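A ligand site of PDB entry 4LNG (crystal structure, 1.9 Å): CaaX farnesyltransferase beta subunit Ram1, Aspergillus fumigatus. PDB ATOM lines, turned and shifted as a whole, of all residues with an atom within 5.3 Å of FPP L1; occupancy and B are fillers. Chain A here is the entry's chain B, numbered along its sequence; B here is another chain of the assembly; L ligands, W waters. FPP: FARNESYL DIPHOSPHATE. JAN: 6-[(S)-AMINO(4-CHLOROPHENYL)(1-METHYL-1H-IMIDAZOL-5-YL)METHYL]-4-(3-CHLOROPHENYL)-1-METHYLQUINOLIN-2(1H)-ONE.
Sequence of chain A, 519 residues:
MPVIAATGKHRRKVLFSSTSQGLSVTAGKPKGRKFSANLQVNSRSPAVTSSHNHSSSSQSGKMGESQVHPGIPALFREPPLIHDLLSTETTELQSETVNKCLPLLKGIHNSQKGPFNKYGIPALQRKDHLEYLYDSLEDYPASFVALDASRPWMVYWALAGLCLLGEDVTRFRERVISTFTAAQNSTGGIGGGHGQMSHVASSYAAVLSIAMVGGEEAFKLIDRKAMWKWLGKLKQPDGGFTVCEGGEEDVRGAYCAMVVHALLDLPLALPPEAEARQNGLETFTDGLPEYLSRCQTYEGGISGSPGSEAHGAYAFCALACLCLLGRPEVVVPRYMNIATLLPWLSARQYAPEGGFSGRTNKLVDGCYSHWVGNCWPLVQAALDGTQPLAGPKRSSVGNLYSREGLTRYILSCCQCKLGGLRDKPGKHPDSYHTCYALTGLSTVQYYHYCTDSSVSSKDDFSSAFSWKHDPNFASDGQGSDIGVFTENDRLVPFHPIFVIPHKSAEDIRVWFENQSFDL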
ATOM      1  N   TRP A 153      18.765  -8.369 -33.495  1.00  0.00           N
ATOM      2  CA  TRP A 153      18.840  -7.239 -32.555  1.00  0.00           C
ATOM      3  C   TRP A 153      19.979  -6.301 -32.940  1.00  0.00           C
ATOM      4  O   TRP A 153      19.822  -5.082 -32.910  1.00  0.00           O
ATOM      5  CB  TRP A 153      19.083  -7.733 -31.124  1.00  0.00           C
ATOM      6  CG  TRP A 153      17.873  -8.021 -30.283  1.00  0.00           C
ATOM      7  CD1 TRP A 153      17.613  -9.163 -29.591  1.00  0.00           C
ATOM      8  CD2 TRP A 153      16.767  -7.129 -30.004  1.00  0.00           C
ATOM      9  NE1 TRP A 153      16.420  -9.054 -28.918  1.00  0.00           N
ATOM     10  CE2 TRP A 153      15.885  -7.825 -29.158  1.00  0.00           C
ATOM     11  CE3 TRP A 153      16.446  -5.824 -30.397  1.00  0.00           C
ATOM     12  CZ2 TRP A 153      14.693  -7.258 -28.691  1.00  0.00           C
ATOM     13  CZ3 TRP A 153      15.276  -5.261 -29.931  1.00  0.00           C
ATOM     14  CH2 TRP A 153      14.408  -5.975 -29.090  1.00  0.00           C
ATOM     15  N   TYR A 204      10.473  -9.043 -33.941  1.00  0.00           N
ATOM     16  CA  TYR A 204      10.354  -7.638 -33.596  1.00  0.00           C
ATOM     17  C   TYR A 204      11.498  -6.819 -34.195  1.00  0.00           C
ATOM     18  O   TYR A 204      11.277  -5.830 -34.887  1.00  0.00           O
ATOM     19  CB  TYR A 204      10.334  -7.517 -32.062  1.00  0.00           C
ATOM     20  CG  TYR A 204      10.436  -6.130 -31.484  1.00  0.00           C
ATOM     21  CD1 TYR A 204       9.288  -5.389 -31.214  1.00  0.00           C
ATOM     22  CD2 TYR A 204      11.666  -5.586 -31.146  1.00  0.00           C
ATOM     23  CE1 TYR A 204       9.376  -4.119 -30.645  1.00  0.00           C
ATOM     24  CE2 TYR A 204      11.756  -4.330 -30.579  1.00  0.00           C
ATOM     25  CZ  TYR A 204      10.606  -3.601 -30.327  1.00  0.00           C
ATOM     26  OH  TYR A 204      10.701  -2.343 -29.774  1.00  0.00           O
ATOM     27  N   ARG A 252       7.823  -9.030 -21.975  1.00  0.00           N
ATOM     28  CA  ARG A 252       8.651  -8.718 -23.139  1.00  0.00           C
ATOM     29  C   ARG A 252       8.106  -9.472 -24.338  1.00  0.00           C
ATOM     30  O   ARG A 252       8.021  -8.924 -25.445  1.00  0.00           O
ATOM     31  CB  ARG A 252      10.113  -9.100 -22.877  1.00  0.00           C
ATOM     32  CG  ARG A 252      10.886  -9.444 -24.132  1.00  0.00           C
ATOM     33  CD  ARG A 252      12.205 -10.132 -23.804  1.00  0.00           C
ATOM     34  NE  ARG A 252      12.006 -11.400 -23.121  1.00  0.00           N
ATOM     35  CZ  ARG A 252      12.714 -12.508 -23.369  1.00  0.00           C
ATOM     36  NH1 ARG A 252      13.666 -12.492 -24.287  1.00  0.00           N
ATOM     37  NH2 ARG A 252      12.458 -13.618 -22.700  1.00  0.00           N
ATOM     38  N   TYR A 255       4.772  -7.763 -25.508  1.00  0.00           N
ATOM     39  CA  TYR A 255       5.043  -6.517 -26.209  1.00  0.00           C
ATOM     40  C   TYR A 255       5.597  -6.735 -27.618  1.00  0.00           C
ATOM     41  O   TYR A 255       5.117  -6.148 -28.583  1.00  0.00           O
ATOM     42  CB  TYR A 255       5.989  -5.629 -25.392  1.00  0.00           C
ATOM     43  CG  TYR A 255       6.618  -4.506 -26.187  1.00  0.00           C
ATOM     44  CD1 TYR A 255       5.888  -3.387 -26.562  1.00  0.00           C
ATOM     45  CD2 TYR A 255       7.959  -4.567 -26.565  1.00  0.00           C
ATOM     46  CE1 TYR A 255       6.473  -2.359 -27.289  1.00  0.00           C
ATOM     47  CE2 TYR A 255       8.547  -3.544 -27.299  1.00  0.00           C
ATOM     48  CZ  TYR A 255       7.803  -2.437 -27.658  1.00  0.00           C
ATOM     49  OH  TYR A 255       8.391  -1.423 -28.387  1.00  0.00           O
ATOM     50  N   CYS A 256       6.612  -7.589 -27.739  1.00  0.00           N
ATOM     51  CA  CYS A 256       7.219  -7.885 -29.024  1.00  0.00           C
ATOM     52  C   CYS A 256       6.202  -8.509 -29.984  1.00  0.00           C
ATOM     53  O   CYS A 256       6.166  -8.154 -31.162  1.00  0.00           O
ATOM     54  CB  CYS A 256       8.430  -8.808 -28.883  1.00  0.00           C
ATOM     55  SG  CYS A 256       9.868  -8.002 -28.133  1.00  0.00           S
ATOM     56  N   HIS A 311      10.181  -3.814 -12.502  1.00  0.00           N
ATOM     57  CA  HIS A 311      11.361  -3.425 -13.260  1.00  0.00           C
ATOM     58  C   HIS A 311      10.988  -2.494 -14.418  1.00  0.00           C
ATOM     59  O   HIS A 311      10.020  -2.748 -15.133  1.00  0.00           O
ATOM     60  CB  HIS A 311      12.080  -4.662 -13.805  1.00  0.00           C
ATOM     61  CG  HIS A 311      13.506  -4.406 -14.176  1.00  0.00           C
ATOM     62  ND1 HIS A 311      13.872  -3.686 -15.297  1.00  0.00           N
ATOM     63  CD2 HIS A 311      14.655  -4.773 -13.569  1.00  0.00           C
ATOM     64  CE1 HIS A 311      15.184  -3.624 -15.355  1.00  0.00           C
ATOM     65  NE2 HIS A 311      15.692  -4.278 -14.325  1.00  0.00           N
ATOM     66  N   ALA A 313      12.139  -2.033 -17.325  1.00  0.00           N
ATOM     67  CA  ALA A 313      12.087  -2.668 -18.639  1.00  0.00           C
ATOM     68  C   ALA A 313      10.703  -3.253 -18.920  1.00  0.00           C
ATOM     69  O   ALA A 313      10.168  -3.107 -20.022  1.00  0.00           O
ATOM     70  CB  ALA A 313      13.111  -3.744 -18.704  1.00  0.00           C
ATOM     71  N   TYR A 314      10.140  -3.918 -17.928  1.00  0.00           N
ATOM     72  CA  TYR A 314       8.838  -4.538 -18.091  1.00  0.00           C
ATOM     73  C   TYR A 314       7.712  -3.533 -17.950  1.00  0.00           C
ATOM     74  O   TYR A 314       6.625  -3.725 -18.497  1.00  0.00           O
ATOM     75  CB  TYR A 314       8.693  -5.695 -17.108  1.00  0.00           C
ATOM     76  CG  TYR A 314       9.728  -6.783 -17.293  1.00  0.00           C
ATOM     77  CD1 TYR A 314       9.857  -7.451 -18.502  1.00  0.00           C
ATOM     78  CD2 TYR A 314      10.567  -7.145 -16.250  1.00  0.00           C
ATOM     79  CE1 TYR A 314      10.792  -8.457 -18.674  1.00  0.00           C
ATOM     80  CE2 TYR A 314      11.507  -8.152 -16.406  1.00  0.00           C
ATOM     81  CZ  TYR A 314      11.616  -8.800 -17.626  1.00  0.00           C
ATOM     82  OH  TYR A 314      12.553  -9.793 -17.780  1.00  0.00           O
ATOM     83  N   CYS A 317       7.341  -2.314 -21.517  1.00  0.00           N
ATOM     84  CA  CYS A 317       6.677  -3.335 -22.334  1.00  0.00           C
ATOM     85  C   CYS A 317       5.179  -3.383 -22.048  1.00  0.00           C
ATOM     86  O   CYS A 317       4.372  -3.412 -22.975  1.00  0.00           O
ATOM     87  CB  CYS A 317       7.302  -4.713 -22.113  1.00  0.00           C
ATOM     88  SG  CYS A 317       9.012  -4.846 -22.700  1.00  0.00           S
ATOM     89  N   GLY A 358      16.734   0.575 -12.951  1.00  0.00           N
ATOM     90  CA  GLY A 358      15.679  -0.322 -13.420  1.00  0.00           C
ATOM     91  C   GLY A 358      14.764  -0.808 -12.307  1.00  0.00           C
ATOM     92  O   GLY A 358      13.581  -1.048 -12.525  1.00  0.00           O
ATOM     93  N   ARG A 359      15.319  -0.940 -11.113  1.00  0.00           N
ATOM     94  CA  ARG A 359      14.537  -1.394  -9.967  1.00  0.00           C
ATOM     95  C   ARG A 359      15.061  -0.806  -8.675  1.00  0.00           C
ATOM     96  O   ARG A 359      16.178  -0.269  -8.623  1.00  0.00           O
ATOM     97  CB  ARG A 359      14.478  -2.927  -9.902  1.00  0.00           C
ATOM     98  CG  ARG A 359      15.813  -3.630 -10.172  1.00  0.00           C
ATOM     99  CD  ARG A 359      15.668  -5.156 -10.043  1.00  0.00           C
ATOM    100  NE  ARG A 359      16.826  -5.866 -10.575  1.00  0.00           N
ATOM    101  CZ  ARG A 359      17.260  -7.043 -10.125  1.00  0.00           C
ATOM    102  NH1 ARG A 359      16.625  -7.649  -9.131  1.00  0.00           N
ATOM    103  NH2 ARG A 359      18.331  -7.606 -10.675  1.00  0.00           N
ATOM    104  N   LYS A 362      18.883  -0.575  -6.956  1.00  0.00           N
ATOM    105  CA  LYS A 362      19.944  -0.944  -7.890  1.00  0.00           C
ATOM    106  C   LYS A 362      20.464   0.311  -8.607  1.00  0.00           C
ATOM    107  O   LYS A 362      20.121   1.419  -8.212  1.00  0.00           O
ATOM    108  CB  LYS A 362      19.501  -2.047  -8.853  1.00  0.00           C
ATOM    109  CG  LYS A 362      19.153  -3.361  -8.121  1.00  0.00           C
ATOM    110  CD  LYS A 362      19.470  -4.596  -8.952  1.00  0.00           C
ATOM    111  CE  LYS A 362      20.973  -4.855  -9.010  1.00  0.00           C
ATOM    112  NZ  LYS A 362      21.283  -5.864 -10.061  1.00  0.00           N
ATOM    113  N   LEU A 363      21.288   0.145  -9.642  1.00  0.00           N
ATOM    114  CA  LEU A 363      22.058   1.282 -10.172  1.00  0.00           C
ATOM    115  C   LEU A 363      21.488   1.904 -11.445  1.00  0.00           C
ATOM    116  O   LEU A 363      20.782   1.246 -12.213  1.00  0.00           O
ATOM    117  CB  LEU A 363      23.514   0.845 -10.433  1.00  0.00           C
ATOM    118  CG  LEU A 363      24.262   0.173  -9.285  1.00  0.00           C
ATOM    119  CD1 LEU A 363      25.579  -0.429  -9.762  1.00  0.00           C
ATOM    120  CD2 LEU A 363      24.502   1.143  -8.146  1.00  0.00           C
ATOM    121  N   ASP A 365      21.514   3.251 -15.285  1.00  0.00           N
ATOM    122  CA  ASP A 365      21.982   2.583 -16.490  1.00  0.00           C
ATOM    123  C   ASP A 365      21.419   3.348 -17.684  1.00  0.00           C
ATOM    124  O   ASP A 365      20.218   3.574 -17.775  1.00  0.00           O
ATOM    125  CB  ASP A 365      21.507   1.130 -16.484  1.00  0.00           C
ATOM    126  CG  ASP A 365      21.919   0.341 -17.728  1.00  0.00           C
ATOM    127  OD1 ASP A 365      22.244   0.944 -18.778  1.00  0.00           O
ATOM    128  OD2 ASP A 365      21.896  -0.906 -17.655  1.00  0.00           O
ATOM    129  N   CYS A 367      20.662   2.629 -20.668  1.00  0.00           N
ATOM    130  CA  CYS A 367      19.620   2.045 -21.509  1.00  0.00           C
ATOM    131  C   CYS A 367      18.224   2.315 -20.956  1.00  0.00           C
ATOM    132  O   CYS A 367      17.243   2.315 -21.700  1.00  0.00           O
ATOM    133  CB  CYS A 367      19.837   0.545 -21.763  1.00  0.00           C
ATOM    134  SG  CYS A 367      19.539  -0.557 -20.354  1.00  0.00           S
ATOM    135  N   TYR A 368      18.129   2.551 -19.652  1.00  0.00           N
ATOM    136  CA  TYR A 368      16.834   2.874 -19.042  1.00  0.00           C
ATOM    137  C   TYR A 368      16.385   4.293 -19.418  1.00  0.00           C
ATOM    138  O   TYR A 368      15.269   4.689 -19.107  1.00  0.00           O
ATOM    139  CB  TYR A 368      16.874   2.654 -17.524  1.00  0.00           C
ATOM    140  CG  TYR A 368      17.199   1.230 -17.159  1.00  0.00           C
ATOM    141  CD1 TYR A 368      16.643   0.172 -17.872  1.00  0.00           C
ATOM    142  CD2 TYR A 368      18.092   0.930 -16.141  1.00  0.00           C
ATOM    143  CE1 TYR A 368      16.954  -1.146 -17.568  1.00  0.00           C
ATOM    144  CE2 TYR A 368      18.408  -0.389 -15.820  1.00  0.00           C
ATOM    145  CZ  TYR A 368      17.830  -1.413 -16.542  1.00  0.00           C
ATOM    146  OH  TYR A 368      18.133  -2.725 -16.248  1.00  0.00           O
ATOM    147  N   TRP A 371      13.895   2.604 -21.612  1.00  0.00           N
ATOM    148  CA  TRP A 371      12.911   1.737 -20.932  1.00  0.00           C
ATOM    149  C   TRP A 371      12.086   2.496 -19.902  1.00  0.00           C
ATOM    150  O   TRP A 371      10.866   2.379 -19.870  1.00  0.00           O
ATOM    151  CB  TRP A 371      13.564   0.492 -20.318  1.00  0.00           C
ATOM    152  CG  TRP A 371      14.336  -0.329 -21.325  1.00  0.00           C
ATOM    153  CD1 TRP A 371      15.690  -0.531 -21.345  1.00  0.00           C
ATOM    154  CD2 TRP A 371      13.803  -1.016 -22.463  1.00  0.00           C
ATOM    155  NE1 TRP A 371      16.023  -1.316 -22.426  1.00  0.00           N
ATOM    156  CE2 TRP A 371      14.890  -1.620 -23.135  1.00  0.00           C
ATOM    157  CE3 TRP A 371      12.524  -1.171 -22.991  1.00  0.00           C
ATOM    158  CZ2 TRP A 371      14.735  -2.377 -24.292  1.00  0.00           C
ATOM    159  CZ3 TRP A 371      12.357  -1.924 -24.144  1.00  0.00           C
ATOM    160  CH2 TRP A 371      13.460  -2.515 -24.778  1.00  0.00           C
ATOM    161  N   TYR A 432      23.741  -1.928 -28.200  1.00  0.00           N
ATOM    162  CA  TYR A 432      22.489  -1.933 -27.437  1.00  0.00           C
ATOM    163  C   TYR A 432      22.376  -0.672 -26.589  1.00  0.00           C
ATOM    164  O   TYR A 432      21.364   0.043 -26.641  1.00  0.00           O
ATOM    165  CB  TYR A 432      22.389  -3.206 -26.573  1.00  0.00           C
ATOM    166  CG  TYR A 432      21.371  -3.120 -25.441  1.00  0.00           C
ATOM    167  CD1 TYR A 432      20.060  -3.530 -25.623  1.00  0.00           C
ATOM    168  CD2 TYR A 432      21.743  -2.662 -24.182  1.00  0.00           C
ATOM    169  CE1 TYR A 432      19.130  -3.462 -24.586  1.00  0.00           C
ATOM    170  CE2 TYR A 432      20.833  -2.583 -23.144  1.00  0.00           C
ATOM    171  CZ  TYR A 432      19.527  -2.983 -23.346  1.00  0.00           C
ATOM    172  OH  TYR A 432      18.626  -2.911 -22.299  1.00  0.00           O
ATOM    173  N   LYS B 159      20.709 -10.454  -6.011  1.00  0.00           N
ATOM    174  CA  LYS B 159      19.583  -9.803  -6.667  1.00  0.00           C
ATOM    175  C   LYS B 159      19.259 -10.390  -8.046  1.00  0.00           C
ATOM    176  O   LYS B 159      18.461  -9.818  -8.791  1.00  0.00           O
ATOM    177  CB  LYS B 159      19.840  -8.296  -6.772  1.00  0.00           C
ATOM    178  CG  LYS B 159      20.137  -7.636  -5.435  1.00  0.00           C
ATOM    179  CD  LYS B 159      20.310  -6.136  -5.544  1.00  0.00           C
ATOM    180  CE  LYS B 159      20.491  -5.508  -4.167  1.00  0.00           C
ATOM    181  NZ  LYS B 159      20.493  -4.019  -4.236  1.00  0.00           N
ATOM    182  N   TYR B 161      17.764 -11.505 -10.996  1.00  0.00           N
ATOM    183  CA  TYR B 161      16.344 -11.444 -11.352  1.00  0.00           C
ATOM    184  C   TYR B 161      15.796 -12.800 -11.789  1.00  0.00           C
ATOM    185  O   TYR B 161      14.689 -13.170 -11.403  1.00  0.00           O
ATOM    186  CB  TYR B 161      16.115 -10.415 -12.468  1.00  0.00           C
ATOM    187  CG  TYR B 161      14.666  -9.961 -12.578  1.00  0.00           C
ATOM    188  CD1 TYR B 161      13.742 -10.694 -13.331  1.00  0.00           C
ATOM    189  CD2 TYR B 161      14.232  -8.818 -11.928  1.00  0.00           C
ATOM    190  CE1 TYR B 161      12.423 -10.285 -13.429  1.00  0.00           C
ATOM    191  CE2 TYR B 161      12.911  -8.396 -12.024  1.00  0.00           C
ATOM    192  CZ  TYR B 161      12.017  -9.131 -12.775  1.00  0.00           C
ATOM    193  OH  TYR B 161      10.711  -8.708 -12.852  1.00  0.00           O
HETATM  194  C1  FPP L   1      17.877  -7.557 -14.860  1.00  0.00           C
HETATM  195  O1  FPP L   1      19.253  -7.705 -15.061  1.00  0.00           O
HETATM  196  C2  FPP L   1      17.115  -6.991 -15.866  1.00  0.00           C
HETATM  197  C3  FPP L   1      15.732  -7.477 -16.183  1.00  0.00           C
HETATM  198  C4  FPP L   1      15.705  -8.979 -16.222  1.00  0.00           C
HETATM  199  C5  FPP L   1      15.235  -6.809 -17.500  1.00  0.00           C
HETATM  200  C6  FPP L   1      15.914  -7.218 -18.827  1.00  0.00           C
HETATM  201  C7  FPP L   1      15.313  -6.922 -20.075  1.00  0.00           C
HETATM  202  C8  FPP L   1      15.224  -5.485 -20.573  1.00  0.00           C
HETATM  203  C10 FPP L   1      16.528  -4.754 -20.428  1.00  0.00           C
HETATM  204  C9  FPP L   1      14.659  -5.389 -21.972  1.00  0.00           C
HETATM  205  C11 FPP L   1      13.399  -6.168 -22.261  1.00  0.00           C
HETATM  206  C12 FPP L   1      12.574  -5.803 -23.314  1.00  0.00           C
HETATM  207  C13 FPP L   1      12.990  -5.997 -24.764  1.00  0.00           C
HETATM  208  C14 FPP L   1      13.830  -7.237 -25.037  1.00  0.00           C
HETATM  209  C15 FPP L   1      11.919  -5.735 -25.778  1.00  0.00           C
HETATM  210  PA  FPP L   1      20.308  -6.857 -14.231  1.00  0.00           P
HETATM  211  O1A FPP L   1      20.274  -7.298 -12.790  1.00  0.00           O
HETATM  212  O2A FPP L   1      21.668  -7.116 -14.809  1.00  0.00           O
HETATM  213  O3A FPP L   1      19.973  -5.340 -14.418  1.00  0.00           O
HETATM  214  PB  FPP L   1      19.497  -4.348 -13.280  1.00  0.00           P
HETATM  215  O1B FPP L   1      20.480  -4.301 -12.129  1.00  0.00           O
HETATM  216  O2B FPP L   1      18.133  -4.718 -12.766  1.00  0.00           O
HETATM  217  O3B FPP L   1      19.452  -2.968 -13.917  1.00  0.00           O
HETATM  218  C1  JAN L   2      19.688  -6.099 -17.739  1.00  0.00           C
HETATM  219  N1  JAN L   2      20.437  -5.293 -18.798  1.00  0.00           N
HETATM  220  C2  JAN L   2      20.502  -4.006 -18.602  1.00  0.00           C
HETATM  221  N2  JAN L   2      21.297  -3.500 -19.434  1.00  0.00           N
HETATM  222  C3  JAN L   2      21.831  -4.371 -20.413  1.00  0.00           C
HETATM  223  C4  JAN L   2      21.386  -5.657 -19.812  1.00  0.00           C
HETATM  224  C5  JAN L   2      21.577  -7.190 -20.441  1.00  0.00           C
HETATM  225  C6  JAN L   2      20.107  -7.669 -20.695  1.00  0.00           C
HETATM  226  C7  JAN L   2      19.281  -6.847 -21.391  1.00  0.00           C
HETATM  227  C8  JAN L   2      18.034  -7.204 -21.936  1.00  0.00           C
HETATM  228  C9  JAN L   2      18.073  -8.724 -21.663  1.00  0.00           C
HETATM  229 CL1  JAN L   2      16.451  -9.329 -22.544  1.00  0.00          CL
HETATM  230  C10 JAN L   2      18.774  -9.506 -21.053  1.00  0.00           C
HETATM  231  C11 JAN L   2      19.970  -8.931 -20.472  1.00  0.00           C
HETATM  232  N3  JAN L   2      21.983  -7.907 -19.275  1.00  0.00           N
HETATM  233  C12 JAN L   2      22.525  -6.894 -21.606  1.00  0.00           C
HETATM  234  C13 JAN L   2      22.131  -7.269 -22.738  1.00  0.00           C
HETATM  235  C14 JAN L   2      23.112  -7.257 -23.707  1.00  0.00           C
HETATM  236  C15 JAN L   2      23.774  -6.604 -21.103  1.00  0.00           C
HETATM  237  C16 JAN L   2      24.883  -6.376 -22.250  1.00  0.00           C
HETATM  238  C17 JAN L   2      24.185  -6.690 -23.604  1.00  0.00           C
HETATM  239  N4  JAN L   2      25.292  -6.601 -24.565  1.00  0.00           N
HETATM  240  C18 JAN L   2      26.688  -5.990 -24.178  1.00  0.00           C
HETATM  241  C19 JAN L   2      24.932  -6.697 -25.871  1.00  0.00           C
HETATM  242  O1  JAN L   2      25.844  -6.496 -26.710  1.00  0.00           O
HETATM  243  C20 JAN L   2      23.643  -7.179 -26.029  1.00  0.00           C
HETATM  244  C21 JAN L   2      22.758  -7.589 -25.096  1.00  0.00           C
HETATM  245  C22 JAN L   2      21.409  -8.053 -25.428  1.00  0.00           C
HETATM  246  C23 JAN L   2      20.259  -7.158 -25.239  1.00  0.00           C
HETATM  247  C24 JAN L   2      19.123  -7.829 -25.650  1.00  0.00           C
HETATM  248 CL2  JAN L   2      17.639  -6.870 -25.444  1.00  0.00          CL
HETATM  249  C25 JAN L   2      18.878  -9.250 -26.077  1.00  0.00           C
HETATM  250  C26 JAN L   2      20.152  -9.864 -26.390  1.00  0.00           C
HETATM  251  C27 JAN L   2      21.246  -9.287 -25.978  1.00  0.00           C
HETATM  252  O   HOH W   1      22.937  -5.169 -16.228  1.00  0.00           O
HETATM  253  O   HOH W   2      23.154  -4.582 -13.327  1.00  0.00           O
HETATM  254  O   HOH W   3      21.708  -2.315 -15.368  1.00  0.00           O
HETATM  255  O   HOH W   4      20.573  -9.461 -16.908  1.00  0.00           O
HETATM  256  O   HOH W   5      18.953  -0.930 -12.179  1.00  0.00           O
HETATM  257  O   HOH W   6      22.097  -2.207 -11.267  1.00  0.00           O
HETATM  258  O   HOH W   7      23.083  -9.183 -15.701  1.00  0.00           O
HETATM  259  O   HOH W   8      19.925  -9.964 -12.537  1.00  0.00           O
HETATM  260  O   HOH W   9      21.476  -8.743  -9.912  1.00  0.00           O
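Water W8 lies within hydrogen-bond range of an oxygen (O1A) of FPP L1 (2.7 Å), the backbone NH of Tyr 161 of chain B (3.1 Å) and the guanidinium group of Arg 359 (3.4 Å). Water W5 lies within hydrogen-bond range of an oxygen (O3B) of FPP L1, the backbone NH (N) of Gly 358 and the backbone carbonyl oxygen (O) of Leu 363. Water W6 bridges O1B of FPP L1 (2.8 Å) and N of Leu 363 (3.0 Å). Water W4 bridges O1 of FPP L1 and N3 of JAN L2. Water W9 lies within hydrogen-bond range of the side-chain amino group (NZ) of Lys 362, the backbone carbonyl oxygen (O) of Lys 159 of chain B, the guanidinium group (NH2) of Arg 359 and an oxygen (O1A) of FPP L1.
Residues that only touch FPP L1: Ala 313 (3.3 Å), Tyr 432 (3.4 Å), Trp 371 (3.5 Å), Arg 252 (3.5 Å), Tyr 314 (3.6 Å), Cys 317 (3.7 Å), Trp 153 (3.8 Å), Cys 256 (3.9 Å) and Tyr 161 of chain B (3.9 Å). Hydrophobic or aromatic side chains within 4 Å of FPP L1: Trp 153, His 311, Ala 313, Tyr 368, Trp 371 and Tyr 161 of chain B. Within 4 Å of FPP L1: Trp 153, Arg 252, Cys 256, His 311, Ala 313, Tyr 314, Cys 317, Arg 359, Lys 362, Tyr 368, Trp 371, Tyr 432 and Tyr 161 of chain B. The nearest printed residue that does not touch FPP L1 is Tyr 255 (4.2 Å).
O of Arg 252 lies within hydrogen-bond range of SG of Cys 256 (3.4 Å). The side-chain hydroxyl of Tyr 432 sits close to the side-chain sulfur of Cys 367. The side-chain hydroxyl (OH) of Tyr 368 sits close to a ring nitrogen (NE2) of His 311 (3.5 Å). A ring nitrogen (ND1) of His 311 is in hydrogen-bond range of the backbone NH (N) of Ala 313, at 3.1 Å. The backbone carbonyl oxygen (O) of Lys 159 of chain B lies within hydrogen-bond range of the guanidinium group (NH1) of Arg 359 (2.9 Å). The backbone carbonyl oxygen (O) of Ala 313 lies within hydrogen-bond range of the side-chain sulfur (SG) of Cys 317, 3.4 Å away. NE1 of Trp 371 lies within hydrogen-bond range of OH of Tyr 432 (3.1 Å).
NE2 of His 311 is in hydrogen-bond range of O2B of FPP L1. The guanidinium group of Arg 359 lies within salt-bridge range of an oxygen (O2B) of FPP L1. An oxygen (O3B) of FPP L1 lies within hydrogen-bond range of the side-chain hydroxyl (OH) of Tyr 368 (2.7 Å). O1B of FPP L1 lies within salt-bridge range of NZ of Lys 362, 2.7 Å away.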
